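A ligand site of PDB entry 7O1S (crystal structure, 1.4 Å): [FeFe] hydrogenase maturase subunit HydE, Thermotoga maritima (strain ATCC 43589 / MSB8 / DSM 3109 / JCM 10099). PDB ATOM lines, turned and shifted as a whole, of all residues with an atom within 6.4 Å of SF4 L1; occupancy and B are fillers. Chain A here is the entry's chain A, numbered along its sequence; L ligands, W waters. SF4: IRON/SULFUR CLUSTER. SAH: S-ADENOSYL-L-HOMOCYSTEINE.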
ATOM      1  N   VAL A  62      22.314  -2.529   4.058  1.00  0.00           N
ATOM      2  CA  VAL A  62      22.132  -1.142   4.488  1.00  0.00           C
ATOM      3  C   VAL A  62      21.733  -1.136   5.948  1.00  0.00           C
ATOM      4  O   VAL A  62      20.851  -1.898   6.363  1.00  0.00           O
ATOM      5  CB  VAL A  62      21.067  -0.461   3.622  1.00  0.00           C
ATOM      6  CG1 VAL A  62      20.713   0.921   4.173  1.00  0.00           C
ATOM      7  CG2 VAL A  62      21.524  -0.365   2.151  1.00  0.00           C
ATOM      8  N   CYS A  63      22.370  -0.268   6.744  1.00  0.00           N
ATOM      9  CA  CYS A  63      21.994  -0.173   8.159  1.00  0.00           C
ATOM     10  C   CYS A  63      22.031   1.261   8.656  1.00  0.00           C
ATOM     11  O   CYS A  63      22.976   2.004   8.365  1.00  0.00           O
ATOM     12  CB  CYS A  63      22.845  -1.065   9.064  1.00  0.00           C
ATOM     13  SG  CYS A  63      22.082  -1.218  10.711  1.00  0.00           S
ATOM     14  N   ARG A  64      21.018   1.624   9.434  1.00  0.00           N
ATOM     15  CA  ARG A  64      20.951   2.945  10.055  1.00  0.00           C
ATOM     16  C   ARG A  64      21.674   3.018  11.396  1.00  0.00           C
ATOM     17  O   ARG A  64      21.870   4.129  11.908  1.00  0.00           O
ATOM     18  CB  ARG A  64      19.487   3.337  10.274  1.00  0.00           C
ATOM     19  CG  ARG A  64      18.803   2.504  11.332  1.00  0.00           C
ATOM     20  CD  ARG A  64      17.322   2.866  11.473  1.00  0.00           C
ATOM     21  NE  ARG A  64      16.658   1.932  12.375  1.00  0.00           N
ATOM     22  CZ  ARG A  64      15.443   2.110  12.878  1.00  0.00           C
ATOM     23  NH1 ARG A  64      14.724   3.182  12.556  1.00  0.00           N
ATOM     24  NH2 ARG A  64      14.931   1.200  13.715  1.00  0.00           N
ATOM     25  N   LYS A  65      22.035   1.895  11.990  1.00  0.00           N
ATOM     26  CA  LYS A  65      22.704   1.881  13.286  1.00  0.00           C
ATOM     27  C   LYS A  65      24.213   1.810  13.110  1.00  0.00           C
ATOM     28  O   LYS A  65      24.736   1.635  12.004  1.00  0.00           O
ATOM     29  CB  LYS A  65      22.182   0.716  14.149  1.00  0.00           C
ATOM     30  CG  LYS A  65      20.823   0.998  14.805  1.00  0.00           C
ATOM     31  CD  LYS A  65      20.404  -0.175  15.711  1.00  0.00           C
ATOM     32  CE  LYS A  65      19.303   0.250  16.687  1.00  0.00           C
ATOM     33  NZ  LYS A  65      18.094   0.817  16.023  1.00  0.00           N
ATOM     34  N   ASN A  66      24.923   1.949  14.226  1.00  0.00           N
ATOM     35  CA  ASN A  66      26.361   2.164  14.224  1.00  0.00           C
ATOM     36  C   ASN A  66      27.050   1.278  15.258  1.00  0.00           C
ATOM     37  O   ASN A  66      28.031   1.691  15.889  1.00  0.00           O
ATOM     38  CB  ASN A  66      26.682   3.647  14.459  1.00  0.00           C
ATOM     39  CG  ASN A  66      27.947   4.081  13.792  1.00  0.00           C
ATOM     40  OD1 ASN A  66      28.362   3.510  12.781  1.00  0.00           O
ATOM     41  ND2 ASN A  66      28.582   5.120  14.330  1.00  0.00           N
ATOM     42  N   CYS A  67      26.546   0.058  15.450  1.00  0.00           N
ATOM     43  CA  CYS A  67      27.124  -0.856  16.452  1.00  0.00           C
ATOM     44  C   CYS A  67      28.630  -0.998  16.246  1.00  0.00           C
ATOM     45  O   CYS A  67      29.106  -1.170  15.119  1.00  0.00           O
ATOM     46  CB  CYS A  67      26.451  -2.222  16.341  1.00  0.00           C
ATOM     47  SG  CYS A  67      24.654  -2.175  16.451  1.00  0.00           S
ATOM     48  N   LEU A  68      29.374  -0.921  17.356  1.00  0.00           N
ATOM     49  CA  LEU A  68      30.826  -0.806  17.271  1.00  0.00           C
ATOM     50  C   LEU A  68      31.495  -2.057  16.736  1.00  0.00           C
ATOM     51  O   LEU A  68      32.619  -1.957  16.214  1.00  0.00           O
ATOM     52  CB  LEU A  68      31.421  -0.449  18.627  1.00  0.00           C
ATOM     53  CG  LEU A  68      31.637   1.039  18.916  1.00  0.00           C
ATOM     54  CD1 LEU A  68      30.324   1.805  18.883  1.00  0.00           C
ATOM     55  CD2 LEU A  68      32.332   1.214  20.263  1.00  0.00           C
ATOM     56  N   TYR A  69      30.859  -3.215  16.863  1.00  0.00           N
ATOM     57  CA  TYR A  69      31.448  -4.480  16.446  1.00  0.00           C
ATOM     58  C   TYR A  69      31.144  -4.839  14.993  1.00  0.00           C
ATOM     59  O   TYR A  69      31.819  -5.715  14.436  1.00  0.00           O
ATOM     60  CB  TYR A  69      30.943  -5.616  17.345  1.00  0.00           C
ATOM     61  CG  TYR A  69      29.448  -5.559  17.634  1.00  0.00           C
ATOM     62  CD1 TYR A  69      28.527  -6.062  16.724  1.00  0.00           C
ATOM     63  CD2 TYR A  69      28.967  -4.983  18.801  1.00  0.00           C
ATOM     64  CE1 TYR A  69      27.154  -6.010  16.972  1.00  0.00           C
ATOM     65  CE2 TYR A  69      27.601  -4.926  19.070  1.00  0.00           C
ATOM     66  CZ  TYR A  69      26.702  -5.438  18.146  1.00  0.00           C
ATOM     67  OH  TYR A  69      25.351  -5.379  18.396  1.00  0.00           O
ATOM     68  N   CYS A  70      30.167  -4.195  14.357  1.00  0.00           N
ATOM     69  CA  CYS A  70      29.548  -4.718  13.146  1.00  0.00           C
ATOM     70  C   CYS A  70      30.089  -4.049  11.890  1.00  0.00           C
ATOM     71  O   CYS A  70      30.090  -2.822  11.776  1.00  0.00           O
ATOM     72  CB  CYS A  70      28.035  -4.526  13.186  1.00  0.00           C
ATOM     73  SG  CYS A  70      27.212  -5.311  11.797  1.00  0.00           S
ATOM     74  N   GLY A  71      30.490  -4.881  10.918  1.00  0.00           N
ATOM     75  CA  GLY A  71      30.962  -4.363   9.645  1.00  0.00           C
ATOM     76  C   GLY A  71      29.914  -3.616   8.835  1.00  0.00           C
ATOM     77  O   GLY A  71      30.282  -2.864   7.938  1.00  0.00           O
ATOM     78  N   LEU A  72      28.628  -3.819   9.138  1.00  0.00           N
ATOM     79  CA  LEU A  72      27.576  -3.098   8.421  1.00  0.00           C
ATOM     80  C   LEU A  72      27.262  -1.745   9.051  1.00  0.00           C
ATOM     81  O   LEU A  72      26.419  -1.014   8.518  1.00  0.00           O
ATOM     82  CB  LEU A  72      26.282  -3.922   8.323  1.00  0.00           C
ATOM     83  CG  LEU A  72      26.347  -5.335   7.752  1.00  0.00           C
ATOM     84  CD1 LEU A  72      24.926  -5.862   7.485  1.00  0.00           C
ATOM     85  CD2 LEU A  72      27.236  -5.459   6.525  1.00  0.00           C
ATOM     86  N   ARG A  73      27.937  -1.383  10.143  1.00  0.00           N
ATOM     87  CA  ARG A  73      27.647  -0.122  10.839  1.00  0.00           C
ATOM     88  C   ARG A  73      27.660   1.047   9.851  1.00  0.00           C
ATOM     89  O   ARG A  73      28.417   1.065   8.885  1.00  0.00           O
ATOM     90  CB  ARG A  73      28.647   0.109  11.967  1.00  0.00           C
ATOM     91  CG  ARG A  73      30.085   0.307  11.491  1.00  0.00           C
ATOM     92  CD  ARG A  73      31.060   0.107  12.646  1.00  0.00           C
ATOM     93  NE  ARG A  73      30.687   0.888  13.832  1.00  0.00           N
ATOM     94  CZ  ARG A  73      31.095   2.123  14.075  1.00  0.00           C
ATOM     95  NH1 ARG A  73      31.918   2.746  13.237  1.00  0.00           N
ATOM     96  NH2 ARG A  73      30.695   2.738  15.181  1.00  0.00           N
ATOM     97  N   ARG A  74      26.791   2.036  10.104  1.00  0.00           N
ATOM     98  CA  ARG A  74      26.569   3.070   9.107  1.00  0.00           C
ATOM     99  C   ARG A  74      27.836   3.870   8.802  1.00  0.00           C
ATOM    100  O   ARG A  74      27.984   4.380   7.676  1.00  0.00           O
ATOM    101  CB  ARG A  74      25.414   4.008   9.495  1.00  0.00           C
ATOM    102  CG  ARG A  74      25.690   4.873  10.696  1.00  0.00           C
ATOM    103  CD  ARG A  74      24.678   6.001  10.889  1.00  0.00           C
ATOM    104  NE  ARG A  74      25.110   6.788  12.036  1.00  0.00           N
ATOM    105  CZ  ARG A  74      24.714   6.554  13.285  1.00  0.00           C
ATOM    106  NH1 ARG A  74      23.848   5.598  13.552  1.00  0.00           N
ATOM    107  NH2 ARG A  74      25.195   7.299  14.284  1.00  0.00           N
ATOM    108  N   SER A 108      18.733  -8.747   7.655  1.00  0.00           N
ATOM    109  CA  SER A 108      19.291  -7.559   7.014  1.00  0.00           C
ATOM    110  C   SER A 108      19.847  -6.622   8.072  1.00  0.00           C
ATOM    111  O   SER A 108      19.597  -6.784   9.271  1.00  0.00           O
ATOM    112  CB  SER A 108      18.220  -6.816   6.212  1.00  0.00           C
ATOM    113  OG  SER A 108      17.178  -6.396   7.063  1.00  0.00           O
ATOM    114  N   GLY A 109      20.589  -5.625   7.600  1.00  0.00           N
ATOM    115  CA  GLY A 109      20.795  -4.436   8.397  1.00  0.00           C
ATOM    116  C   GLY A 109      19.454  -3.760   8.665  1.00  0.00           C
ATOM    117  O   GLY A 109      18.420  -4.094   8.085  1.00  0.00           O
ATOM    118  N   GLU A 110      19.464  -2.803   9.586  1.00  0.00           N
ATOM    119  CA  GLU A 110      18.249  -2.035   9.858  1.00  0.00           C
ATOM    120  C   GLU A 110      18.076  -1.029   8.718  1.00  0.00           C
ATOM    121  O   GLU A 110      18.457   0.136   8.809  1.00  0.00           O
ATOM    122  CB  GLU A 110      18.314  -1.340  11.203  1.00  0.00           C
ATOM    123  CG  GLU A 110      18.185  -2.320  12.365  1.00  0.00           C
ATOM    124  CD  GLU A 110      17.856  -1.620  13.669  1.00  0.00           C
ATOM    125  OE1 GLU A 110      17.619  -0.391  13.650  1.00  0.00           O
ATOM    126  OE2 GLU A 110      17.834  -2.290  14.731  1.00  0.00           O
ATOM    127  N   GLY A 138      16.189  -6.494  13.167  1.00  0.00           N
ATOM    128  CA  GLY A 138      16.559  -5.505  14.164  1.00  0.00           C
ATOM    129  C   GLY A 138      15.374  -4.970  14.941  1.00  0.00           C
ATOM    130  O   GLY A 138      14.307  -5.597  15.066  1.00  0.00           O
ATOM    131  N   GLU A 161      22.734  -9.790  22.377  1.00  0.00           N
ATOM    132  CA  GLU A 161      24.126  -9.343  22.261  1.00  0.00           C
ATOM    133  C   GLU A 161      24.879  -9.388  23.582  1.00  0.00           C
ATOM    134  O   GLU A 161      25.893 -10.093  23.690  1.00  0.00           O
ATOM    135  CB  GLU A 161      24.247  -7.949  21.625  1.00  0.00           C
ATOM    136  CG  GLU A 161      23.281  -7.701  20.457  1.00  0.00           C
ATOM    137  CD  GLU A 161      23.474  -8.620  19.251  1.00  0.00           C
ATOM    138  OE1 GLU A 161      24.272  -9.587  19.288  1.00  0.00           O
ATOM    139  OE2 GLU A 161      22.786  -8.364  18.237  1.00  0.00           O
ATOM    140  N   ARG A 172      26.514  -0.308  21.407  1.00  0.00           N
ATOM    141  CA  ARG A 172      25.365  -0.088  20.534  1.00  0.00           C
ATOM    142  C   ARG A 172      24.817   1.298  20.846  1.00  0.00           C
ATOM    143  O   ARG A 172      23.774   1.446  21.485  1.00  0.00           O
ATOM    144  CB  ARG A 172      24.327  -1.197  20.733  1.00  0.00           C
ATOM    145  CG  ARG A 172      24.943  -2.613  20.699  1.00  0.00           C
ATOM    146  CD  ARG A 172      23.897  -3.727  20.611  1.00  0.00           C
ATOM    147  NE  ARG A 172      23.146  -3.631  19.359  1.00  0.00           N
ATOM    148  CZ  ARG A 172      21.844  -3.391  19.273  1.00  0.00           C
ATOM    149  NH1 ARG A 172      21.107  -3.268  20.379  1.00  0.00           N
ATOM    150  NH2 ARG A 172      21.278  -3.283  18.083  1.00  0.00           N
ATOM    151  N   ARG A 180      16.261  -3.233  23.651  1.00  0.00           N
ATOM    152  CA  ARG A 180      16.385  -4.560  23.052  1.00  0.00           C
ATOM    153  C   ARG A 180      15.478  -5.552  23.759  1.00  0.00           C
ATOM    154  O   ARG A 180      14.767  -6.341  23.116  1.00  0.00           O
ATOM    155  CB  ARG A 180      17.829  -5.027  23.151  1.00  0.00           C
ATOM    156  CG  ARG A 180      18.195  -6.212  22.253  1.00  0.00           C
ATOM    157  CD  ARG A 180      18.500  -5.721  20.874  1.00  0.00           C
ATOM    158  NE  ARG A 180      19.111  -6.736  20.008  1.00  0.00           N
ATOM    159  CZ  ARG A 180      19.326  -6.531  18.714  1.00  0.00           C
ATOM    160  NH1 ARG A 180      18.991  -5.368  18.166  1.00  0.00           N
ATOM    161  NH2 ARG A 180      19.876  -7.488  17.968  1.00  0.00           N
ATOM    162  N   TYR A 303      27.821  -8.990   2.538  1.00  0.00           N
ATOM    163  CA  TYR A 303      27.189  -9.031   3.853  1.00  0.00           C
ATOM    164  C   TYR A 303      28.263  -9.355   4.905  1.00  0.00           C
ATOM    165  O   TYR A 303      28.340 -10.458   5.441  1.00  0.00           O
ATOM    166  CB  TYR A 303      26.045 -10.037   3.852  1.00  0.00           C
ATOM    167  CG  TYR A 303      25.094  -9.876   5.014  1.00  0.00           C
ATOM    168  CD1 TYR A 303      24.157  -8.842   5.038  1.00  0.00           C
ATOM    169  CD2 TYR A 303      25.135 -10.746   6.086  1.00  0.00           C
ATOM    170  CE1 TYR A 303      23.290  -8.684   6.099  1.00  0.00           C
ATOM    171  CE2 TYR A 303      24.273 -10.608   7.155  1.00  0.00           C
ATOM    172  CZ  TYR A 303      23.351  -9.585   7.153  1.00  0.00           C
ATOM    173  OH  TYR A 303      22.499  -9.461   8.217  1.00  0.00           O
ATOM    174  N   LEU A 305      29.343  -8.837   8.118  1.00  0.00           N
ATOM    175  CA  LEU A 305      29.259  -8.591   9.568  1.00  0.00           C
ATOM    176  C   LEU A 305      30.635  -8.667  10.213  1.00  0.00           C
ATOM    177  O   LEU A 305      30.990  -7.828  11.042  1.00  0.00           O
ATOM    178  CB  LEU A 305      28.319  -9.602  10.222  1.00  0.00           C
ATOM    179  CG  LEU A 305      26.887  -9.721   9.705  1.00  0.00           C
ATOM    180  CD1 LEU A 305      26.221 -10.940  10.347  1.00  0.00           C
ATOM    181  CD2 LEU A 305      26.083  -8.467   9.970  1.00  0.00           C
HETATM  182 FE1  SF4 L   1      25.154  -4.575  12.397  1.00  0.00          FE
HETATM  183 FE2  SF4 L   1      23.165  -2.782  11.915  1.00  0.00          FE
HETATM  184 FE3  SF4 L   1      24.025  -3.251  14.476  1.00  0.00          FE
HETATM  185 FE4  SF4 L   1      22.535  -5.254  13.133  1.00  0.00          FE
HETATM  186  S1  SF4 L   1      21.853  -3.137  13.763  1.00  0.00           S
HETATM  187  S2  SF4 L   1      24.467  -5.509  14.370  1.00  0.00           S
HETATM  188  S3  SF4 L   1      23.364  -4.877  11.011  1.00  0.00           S
HETATM  189  S4  SF4 L   1      25.244  -2.296  12.773  1.00  0.00           S
HETATM  190  N   SAH L   2      20.445  -5.913  12.031  1.00  0.00           N
HETATM  191  CA  SAH L   2      19.908  -7.077  12.732  1.00  0.00           C
HETATM  192  CB  SAH L   2      20.284  -8.388  12.035  1.00  0.00           C
HETATM  193  CG  SAH L   2      21.658  -8.493  11.378  1.00  0.00           C
HETATM  194  SD  SAH L   2      23.110  -8.478  12.475  1.00  0.00           S
HETATM  195  C   SAH L   2      20.300  -7.092  14.202  1.00  0.00           C
HETATM  196  O   SAH L   2      19.678  -7.794  15.016  1.00  0.00           O
HETATM  197  OXT SAH L   2      21.252  -6.414  14.625  1.00  0.00           O
HETATM  198  C5' SAH L   2      22.906 -10.193  13.006  1.00  0.00           C
HETATM  199  C4' SAH L   2      23.898 -10.569  14.114  1.00  0.00           C
HETATM  200  O4' SAH L   2      25.236 -10.510  13.675  1.00  0.00           O
HETATM  201  C3' SAH L   2      23.873  -9.666  15.344  1.00  0.00           C
HETATM  202  O3' SAH L   2      22.838 -10.021  16.230  1.00  0.00           O
HETATM  203  C2' SAH L   2      25.241  -9.895  15.971  1.00  0.00           C
HETATM  204  O2' SAH L   2      25.171 -10.802  17.057  1.00  0.00           O
HETATM  205  C1' SAH L   2      26.046 -10.536  14.840  1.00  0.00           C
HETATM  206  N9  SAH L   2      27.328  -9.814  14.648  1.00  0.00           N
HETATM  207  C8  SAH L   2      27.492  -8.517  14.222  1.00  0.00           C
HETATM  208  N7  SAH L   2      28.810  -8.218  14.203  1.00  0.00           N
HETATM  209  C5  SAH L   2      29.501  -9.304  14.642  1.00  0.00           C
HETATM  210  C6  SAH L   2      30.864  -9.554  14.817  1.00  0.00           C
HETATM  211  N6  SAH L   2      31.798  -8.620  14.559  1.00  0.00           N
HETATM  212  N1  SAH L   2      31.257 -10.791  15.292  1.00  0.00           N
HETATM  213  C2  SAH L   2      30.325 -11.776  15.556  1.00  0.00           C
HETATM  214  N3  SAH L   2      28.973 -11.532  15.374  1.00  0.00           N
HETATM  215  C4  SAH L   2      28.573 -10.320  14.916  1.00  0.00           C
HETATM  216  O   HOH W   1      22.927  -5.887  17.175  1.00  0.00           O
HETATM  217  O   HOH W   2      19.450  -4.298  15.682  1.00  0.00           O
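SG of Cys 63 binds FE2 of SF4 L1, at 2.3 Å. An iron atom (FE1) of SF4 L1 is bound by the side-chain sulfur (SG) of Cys 70 (2.3 Å). The backbone NH (N) of Cys 67 sits close to a sulfur (S4) of SF4 L1 (3.8 Å). SG of Cys 67 binds FE3 of SF4 L1, at 2.3 Å. The backbone carbonyl oxygen of Tyr 69 sits at hydrogen-bond distance from a nitrogen (N6) of SAH L2 (2.9 Å). The backbone carbonyl oxygen (O) of Ser 108 sits close to a nitrogen (N) of SAH L2 (3.0 Å). OE2 of Glu 161 is in hydrogen-bond range of O3' of SAH L2 (2.6 Å). The guanidinium group of Arg 180 is in salt-bridge range of an oxygen (O) of SAH L2 (3.0 Å).
OXT of SAH L2 is bound to FE4 of SF4 L1 (2.3 Å).
N of Lys 65 lies close to SG of Cys 63, at 3.4 Å. The side-chain sulfur of Cys 70 sits close to the backbone NH of Leu 72. The backbone carbonyl oxygen (O) of Cys 67 lies within hydrogen-bond range of the guanidinium group (NE) of Arg 73 (2.9 Å). The side-chain sulfur of Cys 67 lies close to the guanidinium group of Arg 172 (3.6 Å). O of Asn 66 is in hydrogen-bond range of NH2 of Arg 73. The side-chain hydroxyl of Tyr 69 is in hydrogen-bond range of the guanidinium group of Arg 172. NZ of Lys 65 lies within salt-bridge range of OE1 of Glu 110. The backbone carbonyl oxygen (O) of Lys 65 is in hydrogen-bond range of the backbone NH (N) of Arg 74, at 2.8 Å.
Lys 65 touches SF4 L1. Tyr 69 touches SF4 L1 (CE1 to S2, 3.8 Å). CD1 of Leu 72 touches S3 of SF4 L1 (3.98 Å). Arg 73 touches SF4 L1. Gly 109 touches SF4 L1 (CA to S3, 3.7 Å). Hydrophobic or aromatic side chains that line SF4 L1: Tyr 69 and Leu 72. Of the 22 residues printed, 8 come within 4 Å of SF4 L1. Along chain A the residues within 4 Å of SF4 L1 span positions 63 to 109. The nearest printed residue that does not touch SF4 L1 is Glu 110 (4.01 Å).
Water W1 lies within hydrogen-bond range of OE2 of Glu 161 (2.7 Å), OH of Tyr 69 (2.8 Å), NE of Arg 172 (3.1 Å) and S2 of SF4 L1 (3.2 Å). Water W2 lies within hydrogen-bond range of the guanidinium group (NH1) of Arg 180 (2.7 Å), the side-chain carboxylate (OE2) of Glu 110 (2.7 Å), the guanidinium group (NH2) of Arg 172 (3.2 Å) and a sulfur (S1) of SF4 L1 (3.3 Å).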
